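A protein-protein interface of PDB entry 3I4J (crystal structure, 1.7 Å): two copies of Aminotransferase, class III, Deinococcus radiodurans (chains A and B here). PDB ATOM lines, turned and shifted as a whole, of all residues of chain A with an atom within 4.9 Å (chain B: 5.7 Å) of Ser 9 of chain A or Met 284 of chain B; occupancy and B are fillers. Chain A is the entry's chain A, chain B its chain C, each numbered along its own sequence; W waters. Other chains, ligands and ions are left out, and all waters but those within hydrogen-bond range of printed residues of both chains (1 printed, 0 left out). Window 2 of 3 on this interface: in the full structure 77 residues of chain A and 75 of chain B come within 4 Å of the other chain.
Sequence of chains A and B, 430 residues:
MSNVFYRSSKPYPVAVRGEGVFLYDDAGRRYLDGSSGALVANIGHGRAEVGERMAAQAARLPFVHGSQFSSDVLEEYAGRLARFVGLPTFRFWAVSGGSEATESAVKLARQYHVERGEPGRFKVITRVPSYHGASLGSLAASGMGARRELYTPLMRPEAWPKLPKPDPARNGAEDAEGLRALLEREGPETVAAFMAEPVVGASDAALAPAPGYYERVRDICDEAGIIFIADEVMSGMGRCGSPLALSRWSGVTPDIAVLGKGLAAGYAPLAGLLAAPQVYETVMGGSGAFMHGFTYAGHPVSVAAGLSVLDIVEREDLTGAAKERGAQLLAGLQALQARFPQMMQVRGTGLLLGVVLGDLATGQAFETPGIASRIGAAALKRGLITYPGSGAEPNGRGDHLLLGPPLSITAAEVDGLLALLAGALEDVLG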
ATOM      1  N   PHE A   5       5.690   0.587 -12.709  1.00  0.00           N
ATOM      2  CA  PHE A   5       6.714  -0.364 -13.135  1.00  0.00           C
ATOM      3  C   PHE A   5       8.041   0.247 -12.694  1.00  0.00           C
ATOM      4  O   PHE A   5       8.610   1.079 -13.402  1.00  0.00           O
ATOM      5  CB  PHE A   5       6.693  -0.527 -14.662  1.00  0.00           C
ATOM      6  CG  PHE A   5       7.501  -1.698 -15.172  1.00  0.00           C
ATOM      7  CD1 PHE A   5       6.902  -2.662 -15.981  1.00  0.00           C
ATOM      8  CD2 PHE A   5       8.858  -1.827 -14.873  1.00  0.00           C
ATOM      9  CE1 PHE A   5       7.641  -3.735 -16.484  1.00  0.00           C
ATOM     10  CE2 PHE A   5       9.605  -2.897 -15.371  1.00  0.00           C
ATOM     11  CZ  PHE A   5       8.991  -3.854 -16.182  1.00  0.00           C
ATOM     12  N   TYR A   6       8.523  -0.149 -11.521  1.00  0.00           N
ATOM     13  CA  TYR A   6       9.781   0.384 -11.010  1.00  0.00           C
ATOM     14  C   TYR A   6      10.950  -0.134 -11.837  1.00  0.00           C
ATOM     15  O   TYR A   6      10.851  -1.169 -12.494  1.00  0.00           O
ATOM     16  CB  TYR A   6       9.955   0.007  -9.534  1.00  0.00           C
ATOM     17  CG  TYR A   6       8.932   0.663  -8.632  1.00  0.00           C
ATOM     18  CD1 TYR A   6       8.982   2.032  -8.361  1.00  0.00           C
ATOM     19  CD2 TYR A   6       7.895  -0.078  -8.077  1.00  0.00           C
ATOM     20  CE1 TYR A   6       8.019   2.644  -7.557  1.00  0.00           C
ATOM     21  CE2 TYR A   6       6.932   0.520  -7.277  1.00  0.00           C
ATOM     22  CZ  TYR A   6       6.996   1.878  -7.020  1.00  0.00           C
ATOM     23  OH  TYR A   6       6.033   2.462  -6.227  1.00  0.00           O
ATOM     24  N   ARG A   7      12.054   0.601 -11.808  1.00  0.00           N
ATOM     25  CA  ARG A   7      13.236   0.232 -12.571  1.00  0.00           C
ATOM     26  C   ARG A   7      13.953  -0.987 -12.015  1.00  0.00           C
ATOM     27  O   ARG A   7      14.699  -1.651 -12.732  1.00  0.00           O
ATOM     28  CB  ARG A   7      14.200   1.416 -12.631  1.00  0.00           C
ATOM     29  CG  ARG A   7      13.633   2.618 -13.345  1.00  0.00           C
ATOM     30  CD  ARG A   7      14.643   3.742 -13.389  1.00  0.00           C
ATOM     31  NE  ARG A   7      14.173   4.861 -14.191  1.00  0.00           N
ATOM     32  CZ  ARG A   7      14.944   5.517 -15.051  1.00  0.00           C
ATOM     33  NH1 ARG A   7      16.206   5.150 -15.205  1.00  0.00           N
ATOM     34  NH2 ARG A   7      14.461   6.533 -15.751  1.00  0.00           N
ATOM     35  N   SER A   8      13.728  -1.278 -10.737  1.00  0.00           N
ATOM     36  CA  SER A   8      14.369  -2.419 -10.094  1.00  0.00           C
ATOM     37  C   SER A   8      13.651  -2.756  -8.802  1.00  0.00           C
ATOM     38  O   SER A   8      12.677  -2.105  -8.431  1.00  0.00           O
ATOM     39  CB  SER A   8      15.834  -2.107  -9.780  1.00  0.00           C
ATOM     40  OG  SER A   8      15.938  -1.260  -8.648  1.00  0.00           O
ATOM     41  N   SER A   9      14.159  -3.769  -8.109  1.00  0.00           N
ATOM     42  CA  SER A   9      13.576  -4.220  -6.856  1.00  0.00           C
ATOM     43  C   SER A   9      13.932  -3.342  -5.659  1.00  0.00           C
ATOM     44  O   SER A   9      13.328  -3.476  -4.597  1.00  0.00           O
ATOM     45  CB  SER A   9      14.009  -5.664  -6.575  1.00  0.00           C
ATOM     46  OG  SER A   9      15.423  -5.786  -6.595  1.00  0.00           O
ATOM     47  N   LYS A  10      14.902  -2.446  -5.820  1.00  0.00           N
ATOM     48  CA  LYS A  10      15.294  -1.584  -4.708  1.00  0.00           C
ATOM     49  C   LYS A  10      14.222  -0.538  -4.414  1.00  0.00           C
ATOM     50  O   LYS A  10      13.319  -0.313  -5.225  1.00  0.00           O
ATOM     51  CB  LYS A  10      16.639  -0.905  -4.998  1.00  0.00           C
ATOM     52  CG  LYS A  10      16.611   0.176  -6.059  1.00  0.00           C
ATOM     53  CD  LYS A  10      18.014   0.741  -6.271  1.00  0.00           C
ATOM     54  CE  LYS A  10      18.051   1.757  -7.405  1.00  0.00           C
ATOM     55  NZ  LYS A  10      19.447   2.204  -7.694  1.00  0.00           N
ATOM     56  N   PRO A  11      14.300   0.113  -3.241  1.00  0.00           N
ATOM     57  CA  PRO A  11      13.314   1.130  -2.872  1.00  0.00           C
ATOM     58  C   PRO A  11      13.398   2.422  -3.677  1.00  0.00           C
ATOM     59  O   PRO A  11      14.483   2.916  -3.993  1.00  0.00           O
ATOM     60  CB  PRO A  11      13.595   1.356  -1.388  1.00  0.00           C
ATOM     61  CG  PRO A  11      15.066   1.139  -1.298  1.00  0.00           C
ATOM     62  CD  PRO A  11      15.262  -0.100  -2.143  1.00  0.00           C
ATOM     63  N   VAL B 279       4.848 -10.652 -15.913  1.00  0.00           N
ATOM     64  CA  VAL B 279       6.019 -10.167 -16.629  1.00  0.00           C
ATOM     65  C   VAL B 279       6.843  -9.231 -15.741  1.00  0.00           C
ATOM     66  O   VAL B 279       8.066  -9.349 -15.670  1.00  0.00           O
ATOM     67  CB  VAL B 279       5.603  -9.436 -17.916  1.00  0.00           C
ATOM     68  CG1 VAL B 279       6.831  -8.873 -18.618  1.00  0.00           C
ATOM     69  CG2 VAL B 279       4.858 -10.408 -18.836  1.00  0.00           C
ATOM     70  N   TYR B 280       6.168  -8.309 -15.064  1.00  0.00           N
ATOM     71  CA  TYR B 280       6.841  -7.364 -14.170  1.00  0.00           C
ATOM     72  C   TYR B 280       7.599  -8.099 -13.061  1.00  0.00           C
ATOM     73  O   TYR B 280       8.780  -7.844 -12.824  1.00  0.00           O
ATOM     74  CB  TYR B 280       5.818  -6.416 -13.535  1.00  0.00           C
ATOM     75  CG  TYR B 280       6.389  -5.504 -12.470  1.00  0.00           C
ATOM     76  CD1 TYR B 280       7.334  -4.530 -12.790  1.00  0.00           C
ATOM     77  CD2 TYR B 280       5.978  -5.611 -11.139  1.00  0.00           C
ATOM     78  CE1 TYR B 280       7.861  -3.683 -11.814  1.00  0.00           C
ATOM     79  CE2 TYR B 280       6.500  -4.771 -10.153  1.00  0.00           C
ATOM     80  CZ  TYR B 280       7.440  -3.810 -10.499  1.00  0.00           C
ATOM     81  OH  TYR B 280       7.965  -2.990  -9.528  1.00  0.00           O
ATOM     82  N   GLU B 281       6.911  -9.014 -12.384  1.00  0.00           N
ATOM     83  CA  GLU B 281       7.518  -9.774 -11.291  1.00  0.00           C
ATOM     84  C   GLU B 281       8.723 -10.603 -11.738  1.00  0.00           C
ATOM     85  O   GLU B 281       9.679 -10.778 -10.981  1.00  0.00           O
ATOM     86  CB  GLU B 281       6.473 -10.688 -10.650  1.00  0.00           C
ATOM     87  CG  GLU B 281       5.327  -9.952  -9.984  1.00  0.00           C
ATOM     88  CD  GLU B 281       4.206 -10.888  -9.566  1.00  0.00           C
ATOM     89  OE1 GLU B 281       4.511 -11.962  -9.003  1.00  0.00           O
ATOM     90  OE2 GLU B 281       3.024 -10.546  -9.792  1.00  0.00           O
ATOM     91  N   THR B 282       8.680 -11.115 -12.963  1.00  0.00           N
ATOM     92  CA  THR B 282       9.779 -11.916 -13.496  1.00  0.00           C
ATOM     93  C   THR B 282      11.032 -11.065 -13.689  1.00  0.00           C
ATOM     94  O   THR B 282      12.144 -11.487 -13.361  1.00  0.00           O
ATOM     95  CB  THR B 282       9.395 -12.553 -14.852  1.00  0.00           C
ATOM     96  OG1 THR B 282       8.356 -13.517 -14.642  1.00  0.00           O
ATOM     97  CG2 THR B 282      10.593 -13.235 -15.496  1.00  0.00           C
ATOM     98  N   VAL B 283      10.847  -9.862 -14.218  1.00  0.00           N
ATOM     99  CA  VAL B 283      11.971  -8.967 -14.450  1.00  0.00           C
ATOM    100  C   VAL B 283      12.499  -8.365 -13.142  1.00  0.00           C
ATOM    101  O   VAL B 283      13.701  -8.141 -13.002  1.00  0.00           O
ATOM    102  CB  VAL B 283      11.589  -7.837 -15.454  1.00  0.00           C
ATOM    103  CG1 VAL B 283      10.399  -7.059 -14.946  1.00  0.00           C
ATOM    104  CG2 VAL B 283      12.766  -6.910 -15.669  1.00  0.00           C
ATOM    105  N   MET B 284      11.612  -8.115 -12.180  1.00  0.00           N
ATOM    106  CA  MET B 284      12.042  -7.556 -10.898  1.00  0.00           C
ATOM    107  C   MET B 284      12.892  -8.570 -10.139  1.00  0.00           C
ATOM    108  O   MET B 284      13.804  -8.201  -9.400  1.00  0.00           O
ATOM    109  CB  MET B 284      10.838  -7.148 -10.044  1.00  0.00           C
ATOM    110  CG  MET B 284      10.134  -5.878 -10.513  1.00  0.00           C
ATOM    111  SD  MET B 284      11.208  -4.399 -10.548  1.00  0.00           S
ATOM    112  CE  MET B 284      11.624  -4.329 -12.298  1.00  0.00           C
ATOM    113  N   GLY B 285      12.588  -9.852 -10.328  1.00  0.00           N
ATOM    114  CA  GLY B 285      13.350 -10.895  -9.665  1.00  0.00           C
ATOM    115  C   GLY B 285      14.722 -11.036 -10.296  1.00  0.00           C
ATOM    116  O   GLY B 285      14.975 -10.505 -11.382  1.00  0.00           O
ATOM    117  N   GLY B 286      15.615 -11.750  -9.619  1.00  0.00           N
ATOM    118  CA  GLY B 286      16.956 -11.938 -10.143  1.00  0.00           C
ATOM    119  C   GLY B 286      17.575 -10.645 -10.642  1.00  0.00           C
ATOM    120  O   GLY B 286      18.174 -10.606 -11.717  1.00  0.00           O
ATOM    121  N   PHE B 290      15.585  -3.192 -14.684  1.00  0.00           N
ATOM    122  CA  PHE B 290      14.978  -3.272 -16.009  1.00  0.00           C
ATOM    123  C   PHE B 290      15.726  -2.421 -17.033  1.00  0.00           C
ATOM    124  O   PHE B 290      16.254  -2.945 -18.012  1.00  0.00           O
ATOM    125  CB  PHE B 290      13.511  -2.840 -15.943  1.00  0.00           C
ATOM    126  CG  PHE B 290      12.808  -2.880 -17.269  1.00  0.00           C
ATOM    127  CD1 PHE B 290      12.795  -4.048 -18.030  1.00  0.00           C
ATOM    128  CD2 PHE B 290      12.152  -1.753 -17.757  1.00  0.00           C
ATOM    129  CE1 PHE B 290      12.138  -4.094 -19.257  1.00  0.00           C
ATOM    130  CE2 PHE B 290      11.491  -1.787 -18.986  1.00  0.00           C
ATOM    131  CZ  PHE B 290      11.484  -2.960 -19.736  1.00  0.00           C
HETATM  132  O   HOH W   1      15.387  -5.697  -9.982  1.00  0.00           O
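Ser 9 of chain A touches just one residue of chain B: Met 284 (3.8 Å). Of the printed residues of chain A, Phe 290 of chain B touches Phe 5 and Arg 7. Of the printed residues of chain B, Arg 7 of chain A touches Phe 290. The nearest printed residue of chain B that does not touch Ser 9 of chain A is Gly 285 of chain B (5.8 Å). The nearest printed residue of chain B that does not touch Phe 5 of chain A is Val 279 of chain B (5.6 Å).
Water W1 lies within hydrogen-bond range of N of Ser 9 of chain A (3.0 Å) and O of Met 284 of chain B (3.0 Å).
No position is printed for both chains. Of the 9 pairs that touch across the chains among the printed residues, none has its exchanged pair printed and touching as well.
The backbone carbonyl oxygen (O) of Tyr 6 of chain A sits close to the side-chain sulfur (SD) of Met 284 of chain B, at 3.8 Å. SD of Met 284 of chain B lies close to O of Ser 8 of chain A (3.4 Å). The backbone carbonyl oxygen of Arg 7 of chain A sits at hydrogen-bond distance from the backbone NH of Phe 290 of chain B, 2.6 Å away.
N of Lys 10 of chain A sits close to OG of Ser 8 of chain A, at 3.2 Å. SD of Met 284 of chain B lies close to OH of Tyr 280 of chain B (3.7 Å).
Hydrophobic or aromatic side chains of chain B within 4 Å of the printed part of chain A: Tyr 280, Val 283, Met 284 and Phe 290. Of the 7 printed residues of chain A, 5 touch a printed residue of chain B. Printed residues of chain A that touch a printed residue of chain B: Phe 5, Tyr 6, Arg 7, Ser 8 and Ser 9. Hydrophobic or aromatic side chains of chain A that line the printed part of chain B: Phe 5 and Tyr 6. Among the printed residues, 9 pairs touch across the chains. Among the printed residues, no Asp or Glu carboxylate lies within 4 Å of a Lys or Arg side-chain nitrogen of the other chain.
Tyr 280 of chain B touches Phe 5 of chain A (CD1 to CG, 3.7 Å). Val 283 of chain B touches Phe 5 of chain A (CG1 to CZ, 3.7 Å). Phe 5 of chain A touches Met 284 of chain B. CE2 of Phe 5 of chain A touches CD2 of Phe 290 of chain B, at 3.7 Å. Tyr 6 of chain A touches Tyr 280 of chain B. O of Met 284 of chain B touches CB of Ser 9 of chain A, at 3.8 Å.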
